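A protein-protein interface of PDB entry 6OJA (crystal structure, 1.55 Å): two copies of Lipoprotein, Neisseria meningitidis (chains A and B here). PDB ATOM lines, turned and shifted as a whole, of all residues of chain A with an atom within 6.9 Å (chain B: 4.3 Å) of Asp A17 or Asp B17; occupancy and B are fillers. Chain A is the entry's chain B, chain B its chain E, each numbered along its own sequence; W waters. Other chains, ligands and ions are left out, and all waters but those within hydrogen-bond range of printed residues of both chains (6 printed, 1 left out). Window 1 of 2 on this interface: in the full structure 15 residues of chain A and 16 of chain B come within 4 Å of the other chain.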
ATOM      1  N   THR A  10     -16.755  18.059 -24.016  1.00  0.00           N
ATOM      2  CA  THR A  10     -17.396  17.334 -22.917  1.00  0.00           C
ATOM      3  C   THR A  10     -16.744  17.777 -21.629  1.00  0.00           C
ATOM      4  O   THR A  10     -15.682  18.374 -21.636  1.00  0.00           O
ATOM      5  CB  THR A  10     -17.263  15.800 -23.019  1.00  0.00           C
ATOM      6  OG1 THR A  10     -15.894  15.428 -22.847  1.00  0.00           O
ATOM      7  CG2 THR A  10     -17.772  15.273 -24.323  1.00  0.00           C
ATOM      8  N   THR A  11     -17.377  17.441 -20.500  1.00  0.00           N
ATOM      9  CA  THR A  11     -16.647  17.497 -19.249  1.00  0.00           C
ATOM     10  C   THR A  11     -15.634  16.348 -19.198  1.00  0.00           C
ATOM     11  O   THR A  11     -15.657  15.414 -19.995  1.00  0.00           O
ATOM     12  CB  THR A  11     -17.612  17.445 -18.055  1.00  0.00           C
ATOM     13  OG1 THR A  11     -18.715  16.574 -18.334  1.00  0.00           O
ATOM     14  CG2 THR A  11     -18.153  18.852 -17.759  1.00  0.00           C
ATOM     15  N   VAL A  12     -14.749  16.412 -18.217  1.00  0.00           N
ATOM     16  CA  VAL A  12     -13.728  15.391 -18.050  1.00  0.00           C
ATOM     17  C   VAL A  12     -14.396  14.087 -17.625  1.00  0.00           C
ATOM     18  O   VAL A  12     -15.402  14.078 -16.896  1.00  0.00           O
ATOM     19  CB  VAL A  12     -12.712  15.896 -17.005  1.00  0.00           C
ATOM     20  CG1 VAL A  12     -11.815  14.784 -16.508  1.00  0.00           C
ATOM     21  CG2 VAL A  12     -11.870  17.041 -17.595  1.00  0.00           C
ATOM     22  N   GLY A  13     -13.855  12.967 -18.080  1.00  0.00           N
ATOM     23  CA  GLY A  13     -14.285  11.670 -17.582  1.00  0.00           C
ATOM     24  C   GLY A  13     -15.295  11.007 -18.497  1.00  0.00           C
ATOM     25  O   GLY A  13     -15.057  10.851 -19.701  1.00  0.00           O
ATOM     26  N   ASP A  14     -16.444  10.622 -17.933  1.00  0.00           N
ATOM     27  CA  ASP A  14     -17.327   9.665 -18.592  1.00  0.00           C
ATOM     28  C   ASP A  14     -17.769  10.114 -19.982  1.00  0.00           C
ATOM     29  O   ASP A  14     -17.729   9.329 -20.932  1.00  0.00           O
ATOM     30  CB  ASP A  14     -18.538   9.307 -17.711  1.00  0.00           C
ATOM     31  CG  ASP A  14     -19.295  10.507 -17.095  1.00  0.00           C
ATOM     32  OD1 ASP A  14     -19.166  11.671 -17.536  1.00  0.00           O
ATOM     33  OD2 ASP A  14     -20.105  10.229 -16.156  1.00  0.00           O
ATOM     34  N   PHE A  15     -18.215  11.367 -20.142  1.00  0.00           N
ATOM     35  CA  PHE A  15     -18.715  11.768 -21.454  1.00  0.00           C
ATOM     36  C   PHE A  15     -17.596  11.821 -22.499  1.00  0.00           C
ATOM     37  O   PHE A  15     -17.848  11.584 -23.691  1.00  0.00           O
ATOM     38  CB  PHE A  15     -19.420  13.131 -21.354  1.00  0.00           C
ATOM     39  CG  PHE A  15     -20.707  13.103 -20.564  1.00  0.00           C
ATOM     40  CD1 PHE A  15     -21.609  12.064 -20.710  1.00  0.00           C
ATOM     41  CD2 PHE A  15     -21.025  14.150 -19.705  1.00  0.00           C
ATOM     42  CE1 PHE A  15     -22.814  12.040 -19.997  1.00  0.00           C
ATOM     43  CE2 PHE A  15     -22.204  14.139 -18.999  1.00  0.00           C
ATOM     44  CZ  PHE A  15     -23.110  13.092 -19.138  1.00  0.00           C
ATOM     45  N   GLY A  16     -16.375  12.157 -22.077  1.00  0.00           N
ATOM     46  CA  GLY A  16     -15.231  12.114 -22.983  1.00  0.00           C
ATOM     47  C   GLY A  16     -14.871  10.698 -23.383  1.00  0.00           C
ATOM     48  O   GLY A  16     -14.554  10.433 -24.548  1.00  0.00           O
ATOM     49  N   ASP A  17     -14.949   9.769 -22.435  1.00  0.00           N
ATOM     50  CA  ASP A  17     -14.678   8.370 -22.753  1.00  0.00           C
ATOM     51  C   ASP A  17     -15.677   7.838 -23.771  1.00  0.00           C
ATOM     52  O   ASP A  17     -15.308   7.083 -24.672  1.00  0.00           O
ATOM     53  CB  ASP A  17     -14.691   7.518 -21.483  1.00  0.00           C
ATOM     54  CG  ASP A  17     -13.442   7.717 -20.630  1.00  0.00           C
ATOM     55  OD1 ASP A  17     -12.353   7.925 -21.207  1.00  0.00           O
ATOM     56  OD2 ASP A  17     -13.568   7.662 -19.387  1.00  0.00           O
ATOM     57  N   MET A  18     -16.945   8.239 -23.679  1.00  0.00           N
ATOM     58  CA  MET A  18     -17.898   7.796 -24.688  1.00  0.00           C
ATOM     59  C   MET A  18     -17.410   8.148 -26.084  1.00  0.00           C
ATOM     60  O   MET A  18     -17.530   7.345 -27.018  1.00  0.00           O
ATOM     61  CB  MET A  18     -19.265   8.436 -24.459  1.00  0.00           C
ATOM     62  CG  MET A  18     -19.957   7.971 -23.213  1.00  0.00           C
ATOM     63  SD  MET A  18     -21.517   8.854 -22.986  1.00  0.00           S
ATOM     64  CE  MET A  18     -21.832   8.437 -21.291  1.00  0.00           C
ATOM     65  N   VAL A  19     -16.918   9.377 -26.258  1.00  0.00           N
ATOM     66  CA  VAL A  19     -16.454   9.833 -27.563  1.00  0.00           C
ATOM     67  C   VAL A  19     -15.249   9.027 -28.013  1.00  0.00           C
ATOM     68  O   VAL A  19     -15.231   8.490 -29.128  1.00  0.00           O
ATOM     69  CB  VAL A  19     -16.125  11.334 -27.528  1.00  0.00           C
ATOM     70  CG1 VAL A  19     -15.544  11.792 -28.863  1.00  0.00           C
ATOM     71  CG2 VAL A  19     -17.369  12.126 -27.206  1.00  0.00           C
ATOM     72  N   LYS A  20     -14.229   8.929 -27.151  1.00  0.00           N
ATOM     73  CA  LYS A  20     -12.951   8.356 -27.577  1.00  0.00           C
ATOM     74  C   LYS A  20     -13.036   6.845 -27.701  1.00  0.00           C
ATOM     75  O   LYS A  20     -12.341   6.260 -28.544  1.00  0.00           O
ATOM     76  CB  LYS A  20     -11.838   8.717 -26.593  1.00  0.00           C
ATOM     77  CG  LYS A  20     -11.535  10.208 -26.471  1.00  0.00           C
ATOM     78  CD  LYS A  20     -11.208  10.918 -27.782  1.00  0.00           C
ATOM     79  CE  LYS A  20      -9.933  10.367 -28.416  1.00  0.00           C
ATOM     80  NZ  LYS A  20      -9.525  11.164 -29.621  1.00  0.00           N
ATOM     81  N   GLU A  21     -13.889   6.201 -26.907  1.00  0.00           N
ATOM     82  CA  GLU A  21     -13.933   4.737 -26.868  1.00  0.00           C
ATOM     83  C   GLU A  21     -14.889   4.149 -27.886  1.00  0.00           C
ATOM     84  O   GLU A  21     -14.671   3.023 -28.346  1.00  0.00           O
ATOM     85  CB  GLU A  21     -14.313   4.257 -25.469  1.00  0.00           C
ATOM     86  CG  GLU A  21     -13.268   4.576 -24.448  1.00  0.00           C
ATOM     87  CD  GLU A  21     -13.607   4.109 -23.071  1.00  0.00           C
ATOM     88  OE1 GLU A  21     -14.814   3.956 -22.762  1.00  0.00           O
ATOM     89  OE2 GLU A  21     -12.658   3.877 -22.282  1.00  0.00           O
ATOM     90  N   GLN A  22     -15.935   4.872 -28.274  1.00  0.00           N
ATOM     91  CA  GLN A  22     -16.991   4.267 -29.078  1.00  0.00           C
ATOM     92  C   GLN A  22     -17.403   5.176 -30.236  1.00  0.00           C
ATOM     93  O   GLN A  22     -17.379   4.766 -31.400  1.00  0.00           O
ATOM     94  CB  GLN A  22     -18.183   3.930 -28.175  1.00  0.00           C
ATOM     95  CG  GLN A  22     -19.393   3.338 -28.869  1.00  0.00           C
ATOM     96  CD  GLN A  22     -19.175   1.933 -29.356  1.00  0.00           C
ATOM     97  OE1 GLN A  22     -18.306   1.199 -28.852  1.00  0.00           O
ATOM     98  NE2 GLN A  22     -19.973   1.534 -30.342  1.00  0.00           N
ATOM     99  N   ILE A  23     -17.777   6.419 -29.944  1.00  0.00           N
ATOM    100  CA  ILE A  23     -18.366   7.269 -30.976  1.00  0.00           C
ATOM    101  C   ILE A  23     -17.359   7.602 -32.075  1.00  0.00           C
ATOM    102  O   ILE A  23     -17.704   7.610 -33.259  1.00  0.00           O
ATOM    103  CB  ILE A  23     -18.929   8.553 -30.344  1.00  0.00           C
ATOM    104  CG1 ILE A  23     -19.963   8.206 -29.268  1.00  0.00           C
ATOM    105  CG2 ILE A  23     -19.521   9.455 -31.425  1.00  0.00           C
ATOM    106  CD1 ILE A  23     -21.212   7.532 -29.783  1.00  0.00           C
ATOM    107  N   LEU A  36     -11.721  16.019 -29.691  1.00  0.00           N
ATOM    108  CA  LEU A  36     -12.389  16.135 -28.400  1.00  0.00           C
ATOM    109  C   LEU A  36     -11.657  17.178 -27.579  1.00  0.00           C
ATOM    110  O   LEU A  36     -10.435  17.103 -27.415  1.00  0.00           O
ATOM    111  CB  LEU A  36     -12.393  14.822 -27.647  1.00  0.00           C
ATOM    112  CG  LEU A  36     -12.944  14.874 -26.208  1.00  0.00           C
ATOM    113  CD1 LEU A  36     -14.450  15.202 -26.184  1.00  0.00           C
ATOM    114  CD2 LEU A  36     -12.659  13.576 -25.453  1.00  0.00           C
ATOM    115  N   GLU A  38     -11.935  18.684 -23.686  1.00  0.00           N
ATOM    116  CA  GLU A  38     -12.555  18.467 -22.382  1.00  0.00           C
ATOM    117  C   GLU A  38     -12.453  19.729 -21.538  1.00  0.00           C
ATOM    118  O   GLU A  38     -11.496  20.502 -21.644  1.00  0.00           O
ATOM    119  CB  GLU A  38     -11.928  17.278 -21.642  1.00  0.00           C
ATOM    120  CG  GLU A  38     -12.283  15.937 -22.314  1.00  0.00           C
ATOM    121  CD  GLU A  38     -11.976  14.697 -21.479  1.00  0.00           C
ATOM    122  OE1 GLU A  38     -11.337  14.803 -20.415  1.00  0.00           O
ATOM    123  OE2 GLU A  38     -12.393  13.596 -21.896  1.00  0.00           O
ATOM    124  N   SER A 180     -15.472  10.940 -11.634  1.00  0.00           N
ATOM    125  CA  SER A 180     -14.081  11.270 -11.910  1.00  0.00           C
ATOM    126  C   SER A 180     -13.259  11.494 -10.647  1.00  0.00           C
ATOM    127  O   SER A 180     -12.027  11.509 -10.720  1.00  0.00           O
ATOM    128  CB  SER A 180     -14.013  12.514 -12.782  1.00  0.00           C
ATOM    129  OG  SER A 180     -14.343  12.234 -14.124  1.00  0.00           O
ATOM    130  N   TYR A 228     -22.338  -1.164 -25.132  1.00  0.00           N
ATOM    131  CA  TYR A 228     -21.153  -0.629 -24.468  1.00  0.00           C
ATOM    132  C   TYR A 228     -21.539   0.142 -23.218  1.00  0.00           C
ATOM    133  O   TYR A 228     -20.937  -0.031 -22.154  1.00  0.00           O
ATOM    134  CB  TYR A 228     -20.375   0.257 -25.458  1.00  0.00           C
ATOM    135  CG  TYR A 228     -19.556   1.398 -24.880  1.00  0.00           C
ATOM    136  CD1 TYR A 228     -18.246   1.220 -24.457  1.00  0.00           C
ATOM    137  CD2 TYR A 228     -20.068   2.686 -24.832  1.00  0.00           C
ATOM    138  CE1 TYR A 228     -17.493   2.273 -23.961  1.00  0.00           C
ATOM    139  CE2 TYR A 228     -19.327   3.738 -24.335  1.00  0.00           C
ATOM    140  CZ  TYR A 228     -18.049   3.549 -23.913  1.00  0.00           C
ATOM    141  OH  TYR A 228     -17.327   4.603 -23.425  1.00  0.00           O
ATOM    142  N   ARG A 232     -20.169  -0.203 -19.325  1.00  0.00           N
ATOM    143  CA  ARG A 232     -19.171   0.807 -19.002  1.00  0.00           C
ATOM    144  C   ARG A 232     -19.690   1.760 -17.935  1.00  0.00           C
ATOM    145  O   ARG A 232     -18.929   2.190 -17.057  1.00  0.00           O
ATOM    146  CB  ARG A 232     -18.791   1.585 -20.255  1.00  0.00           C
ATOM    147  CG  ARG A 232     -17.640   2.568 -20.064  1.00  0.00           C
ATOM    148  CD  ARG A 232     -16.301   1.862 -19.995  1.00  0.00           C
ATOM    149  NE  ARG A 232     -15.170   2.763 -20.192  1.00  0.00           N
ATOM    150  CZ  ARG A 232     -14.343   3.211 -19.248  1.00  0.00           C
ATOM    151  NH1 ARG A 232     -14.496   2.875 -17.973  1.00  0.00           N
ATOM    152  NH2 ARG A 232     -13.328   3.989 -19.590  1.00  0.00           N
ATOM    153  N   PHE A 233     -20.977   2.094 -18.001  1.00  0.00           N
ATOM    154  CA  PHE A 233     -21.594   3.110 -17.143  1.00  0.00           C
ATOM    155  C   PHE A 233     -22.741   2.486 -16.351  1.00  0.00           C
ATOM    156  O   PHE A 233     -23.922   2.797 -16.537  1.00  0.00           O
ATOM    157  CB  PHE A 233     -22.045   4.281 -17.997  1.00  0.00           C
ATOM    158  CG  PHE A 233     -20.940   4.839 -18.865  1.00  0.00           C
ATOM    159  CD1 PHE A 233     -19.853   5.468 -18.301  1.00  0.00           C
ATOM    160  CD2 PHE A 233     -20.984   4.696 -20.235  1.00  0.00           C
ATOM    161  CE1 PHE A 233     -18.836   5.954 -19.084  1.00  0.00           C
ATOM    162  CE2 PHE A 233     -19.975   5.178 -21.014  1.00  0.00           C
ATOM    163  CZ  PHE A 233     -18.901   5.805 -20.442  1.00  0.00           C
ATOM    164  N   GLY B  13      -9.223   5.509 -22.703  1.00  0.00           N
ATOM    165  CA  GLY B  13      -9.793   4.941 -21.495  1.00  0.00           C
ATOM    166  C   GLY B  13      -8.936   5.204 -20.263  1.00  0.00           C
ATOM    167  O   GLY B  13      -8.580   6.357 -19.981  1.00  0.00           O
ATOM    168  N   ASP B  14      -8.617   4.130 -19.516  1.00  0.00           N
ATOM    169  CA  ASP B  14      -8.150   4.294 -18.145  1.00  0.00           C
ATOM    170  C   ASP B  14      -6.888   5.151 -18.048  1.00  0.00           C
ATOM    171  O   ASP B  14      -6.812   6.044 -17.195  1.00  0.00           O
ATOM    172  CB  ASP B  14      -7.968   2.930 -17.443  1.00  0.00           C
ATOM    173  CG  ASP B  14      -7.188   1.891 -18.227  1.00  0.00           C
ATOM    174  OD1 ASP B  14      -6.468   2.196 -19.184  1.00  0.00           O
ATOM    175  OD2 ASP B  14      -7.288   0.705 -17.787  1.00  0.00           O
ATOM    176  N   PHE B  15      -5.868   4.880 -18.865  1.00  0.00           N
ATOM    177  CA  PHE B  15      -4.631   5.644 -18.723  1.00  0.00           C
ATOM    178  C   PHE B  15      -4.840   7.118 -19.074  1.00  0.00           C
ATOM    179  O   PHE B  15      -4.189   7.996 -18.494  1.00  0.00           O
ATOM    180  CB  PHE B  15      -3.544   5.020 -19.594  1.00  0.00           C
ATOM    181  CG  PHE B  15      -3.081   3.661 -19.139  1.00  0.00           C
ATOM    182  CD1 PHE B  15      -2.977   3.332 -17.788  1.00  0.00           C
ATOM    183  CD2 PHE B  15      -2.735   2.718 -20.069  1.00  0.00           C
ATOM    184  CE1 PHE B  15      -2.535   2.087 -17.397  1.00  0.00           C
ATOM    185  CE2 PHE B  15      -2.275   1.457 -19.677  1.00  0.00           C
ATOM    186  CZ  PHE B  15      -2.186   1.149 -18.346  1.00  0.00           C
ATOM    187  N   GLY B  16      -5.729   7.403 -20.013  1.00  0.00           N
ATOM    188  CA  GLY B  16      -6.053   8.790 -20.311  1.00  0.00           C
ATOM    189  C   GLY B  16      -6.811   9.461 -19.186  1.00  0.00           C
ATOM    190  O   GLY B  16      -6.571  10.631 -18.876  1.00  0.00           O
ATOM    191  N   ASP B  17      -7.751   8.747 -18.570  1.00  0.00           N
ATOM    192  CA  ASP B  17      -8.468   9.331 -17.444  1.00  0.00           C
ATOM    193  C   ASP B  17      -7.529   9.676 -16.297  1.00  0.00           C
ATOM    194  O   ASP B  17      -7.718  10.692 -15.617  1.00  0.00           O
ATOM    195  CB  ASP B  17      -9.568   8.382 -17.001  1.00  0.00           C
ATOM    196  CG  ASP B  17     -10.777   8.442 -17.933  1.00  0.00           C
ATOM    197  OD1 ASP B  17     -11.022   9.523 -18.514  1.00  0.00           O
ATOM    198  OD2 ASP B  17     -11.439   7.420 -18.086  1.00  0.00           O
ATOM    199  N   MET B  18      -6.513   8.846 -16.047  1.00  0.00           N
ATOM    200  CA  MET B  18      -5.552   9.191 -15.008  1.00  0.00           C
ATOM    201  C   MET B  18      -4.962  10.564 -15.245  1.00  0.00           C
ATOM    202  O   MET B  18      -4.775  11.334 -14.293  1.00  0.00           O
ATOM    203  CB  MET B  18      -4.430   8.178 -14.946  1.00  0.00           C
ATOM    204  CG  MET B  18      -4.866   6.819 -14.446  1.00  0.00           C
ATOM    205  SD  MET B  18      -3.513   5.624 -14.597  1.00  0.00           S
ATOM    206  CE  MET B  18      -4.455   4.129 -14.424  1.00  0.00           C
ATOM    207  N   VAL B  19      -4.601  10.859 -16.495  1.00  0.00           N
ATOM    208  CA  VAL B  19      -4.021  12.155 -16.827  1.00  0.00           C
ATOM    209  C   VAL B  19      -5.042  13.267 -16.605  1.00  0.00           C
ATOM    210  O   VAL B  19      -4.769  14.246 -15.895  1.00  0.00           O
ATOM    211  CB  VAL B  19      -3.494  12.152 -18.271  1.00  0.00           C
ATOM    212  CG1 VAL B  19      -3.002  13.561 -18.655  1.00  0.00           C
ATOM    213  CG2 VAL B  19      -2.369  11.118 -18.440  1.00  0.00           C
ATOM    214  N   LYS B  20      -6.232  13.127 -17.195  1.00  0.00           N
ATOM    215  CA  LYS B  20      -7.184  14.236 -17.164  1.00  0.00           C
ATOM    216  C   LYS B  20      -7.720  14.463 -15.756  1.00  0.00           C
ATOM    217  O   LYS B  20      -7.975  15.609 -15.358  1.00  0.00           O
ATOM    218  CB  LYS B  20      -8.332  13.983 -18.144  1.00  0.00           C
ATOM    219  CG  LYS B  20      -7.963  13.924 -19.623  1.00  0.00           C
ATOM    220  CD  LYS B  20      -7.261  15.164 -20.132  1.00  0.00           C
ATOM    221  CE  LYS B  20      -8.107  16.417 -19.973  1.00  0.00           C
ATOM    222  NZ  LYS B  20      -7.382  17.617 -20.490  1.00  0.00           N
ATOM    223  N   GLU B  21      -7.907  13.385 -14.983  1.00  0.00           N
ATOM    224  CA  GLU B  21      -8.618  13.493 -13.716  1.00  0.00           C
ATOM    225  C   GLU B  21      -7.718  13.759 -12.525  1.00  0.00           C
ATOM    226  O   GLU B  21      -8.219  14.177 -11.475  1.00  0.00           O
ATOM    227  CB  GLU B  21      -9.423  12.211 -13.458  1.00  0.00           C
ATOM    228  CG  GLU B  21     -10.494  11.963 -14.517  1.00  0.00           C
ATOM    229  CD  GLU B  21     -11.263  10.662 -14.346  1.00  0.00           C
ATOM    230  OE1 GLU B  21     -10.729   9.702 -13.729  1.00  0.00           O
ATOM    231  OE2 GLU B  21     -12.410  10.609 -14.847  1.00  0.00           O
ATOM    232  N   TYR B 228      -6.692   8.225  -5.252  1.00  0.00           N
ATOM    233  CA  TYR B 228      -7.585   8.256  -6.407  1.00  0.00           C
ATOM    234  C   TYR B 228      -7.571   6.921  -7.149  1.00  0.00           C
ATOM    235  O   TYR B 228      -8.626   6.374  -7.487  1.00  0.00           O
ATOM    236  CB  TYR B 228      -7.181   9.420  -7.326  1.00  0.00           C
ATOM    237  CG  TYR B 228      -7.519   9.255  -8.794  1.00  0.00           C
ATOM    238  CD1 TYR B 228      -8.746   9.648  -9.307  1.00  0.00           C
ATOM    239  CD2 TYR B 228      -6.585   8.740  -9.675  1.00  0.00           C
ATOM    240  CE1 TYR B 228      -9.042   9.507 -10.670  1.00  0.00           C
ATOM    241  CE2 TYR B 228      -6.869   8.598 -11.027  1.00  0.00           C
ATOM    242  CZ  TYR B 228      -8.089   8.988 -11.514  1.00  0.00           C
ATOM    243  OH  TYR B 228      -8.391   8.837 -12.843  1.00  0.00           O
ATOM    244  N   ARG B 232     -10.773   4.723  -8.238  1.00  0.00           N
ATOM    245  CA  ARG B 232     -11.226   4.767  -9.620  1.00  0.00           C
ATOM    246  C   ARG B 232     -10.949   3.468 -10.353  1.00  0.00           C
ATOM    247  O   ARG B 232     -11.687   3.115 -11.277  1.00  0.00           O
ATOM    248  CB  ARG B 232     -10.535   5.934 -10.333  1.00  0.00           C
ATOM    249  CG  ARG B 232     -10.986   6.241 -11.770  1.00  0.00           C
ATOM    250  CD  ARG B 232     -12.313   6.982 -11.793  1.00  0.00           C
ATOM    251  NE  ARG B 232     -12.560   7.676 -13.060  1.00  0.00           N
ATOM    252  CZ  ARG B 232     -13.415   7.281 -14.004  1.00  0.00           C
ATOM    253  NH1 ARG B 232     -14.138   6.175 -13.861  1.00  0.00           N
ATOM    254  NH2 ARG B 232     -13.581   8.015 -15.096  1.00  0.00           N
HETATM  255  O   HOH W   1     -10.972   7.588 -23.451  1.00  0.00           O
HETATM  256  O   HOH W   2      -9.986  13.032  -9.429  1.00  0.00           O
HETATM  257  O   HOH W   3      -9.112  19.795 -19.969  1.00  0.00           O
HETATM  258  O   HOH W   4     -15.538   7.059 -17.395  1.00  0.00           O
HETATM  259  O   HOH W   5      -9.502   8.836 -21.351  1.00  0.00           O
HETATM  260  O   HOH W   6     -11.415   4.794 -17.264  1.00  0.00           O
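OH of Tyr A228 lies within hydrogen-bond range of OE1 of Glu A21. The backbone carbonyl oxygen (O) of Asp B17 is in hydrogen-bond range of the side-chain hydroxyl (OH) of Tyr B228 (3.4 Å). O of Val A12 lies within hydrogen-bond range of OG of Ser A180 (3.5 Å). The side-chain carboxylate (OD2) of Asp B17 is in salt-bridge range of the guanidinium group (NH2) of Arg B232 (3.7 Å). The side-chain hydroxyl (OH) of Tyr A228 sits at hydrogen-bond distance from the backbone carbonyl oxygen (O) of Asp A17. The side-chain hydroxyl (OH) of Tyr B228 lies within hydrogen-bond range of the side-chain carboxylate (OE1) of Glu B21, at 2.6 Å.
Water W1 lies within hydrogen-bond range of the side-chain carboxylate of Asp A17 (2.7 Å) and the backbone NH of Gly B13 (2.8 Å). Water W6 bridges OD2 of Asp B17 and NH2 of Arg A232. Water W3 lies within hydrogen-bond range of NZ of Lys B20 and O of Glu A38. Water W2 bridges O of Ser A180 (2.9 Å) and O of Glu B21 (2.9 Å). Water W4 bridges OD2 of Asp A17 (2.9 Å) and NH2 of Arg B232 (3.2 Å). Water W5 lies within hydrogen-bond range of the backbone carbonyl oxygen of Gly B13 (3.0 Å), the side-chain carboxylate of Asp A17 (3.0 Å) and the backbone NH of Asp B17 (3.3 Å).
Gly A13 touches Glu B21, and with the chains exchanged Glu A21 touches Gly B13. Asp A17 touches Gly B13, but with the chains exchanged Gly A13 does not touch Asp B17 (4.02 Å). Asp A17 touches its own counterpart, Asp B17.
Of the printed residues of chain B, Asp A17 touches Gly B13 (3.9 Å) and Asp B17 (2.5 Å). Of the printed residues of chain A, Asp B17 touches Asp A17. Printed residues of chain A within 4 Å of Lys B20: Val A12 (3.9 Å) and Glu A38 (3.6 Å). Of the printed residues of chain A, Glu B21 touches Val A12 (3.7 Å), Gly A13 (3.5 Å) and Ser A180 (2.6 Å). Printed residues of chain B within 4 Å of Val A12: Lys B20 (3.9 Å) and Glu B21 (3.7 Å). Of the printed residues of chain B, Gly A13 touches Glu B21. Arg B232 touches none of the printed residues of chain A. Thr A10 touches none of the printed residues of chain B. The nearest printed residue of chain A that does not touch Lys B20 is Gly A13 (5.6 Å).
Of the 20 printed residues of chain A, 6 touch a printed residue of chain B. Hydrophobic or aromatic side chains of chain A within 4 Å of the printed part of chain B: Val A12. Of the 11 printed residues of chain B, 5 touch a printed residue of chain A. Along chain B the printed residues that touch a printed residue of chain A span positions 13 to 228. Among the printed residues, 9 pairs touch across the chains.
OD2 of Asp A17 lies close to OD2 of Asp B17, 2.5 Å away. OE2 of Glu B21 is in hydrogen-bond range of OG of Ser A180 (2.6 Å).
Among the printed residues, merely in contact across the chains: Glu A21 with Gly B13, Gly A13 with Glu B21, Glu A38 with Lys B20, Ser A180 with Tyr B228, Val A12 with Glu B21, Val A12 with Lys B20 and Asp A17 with Gly B13.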
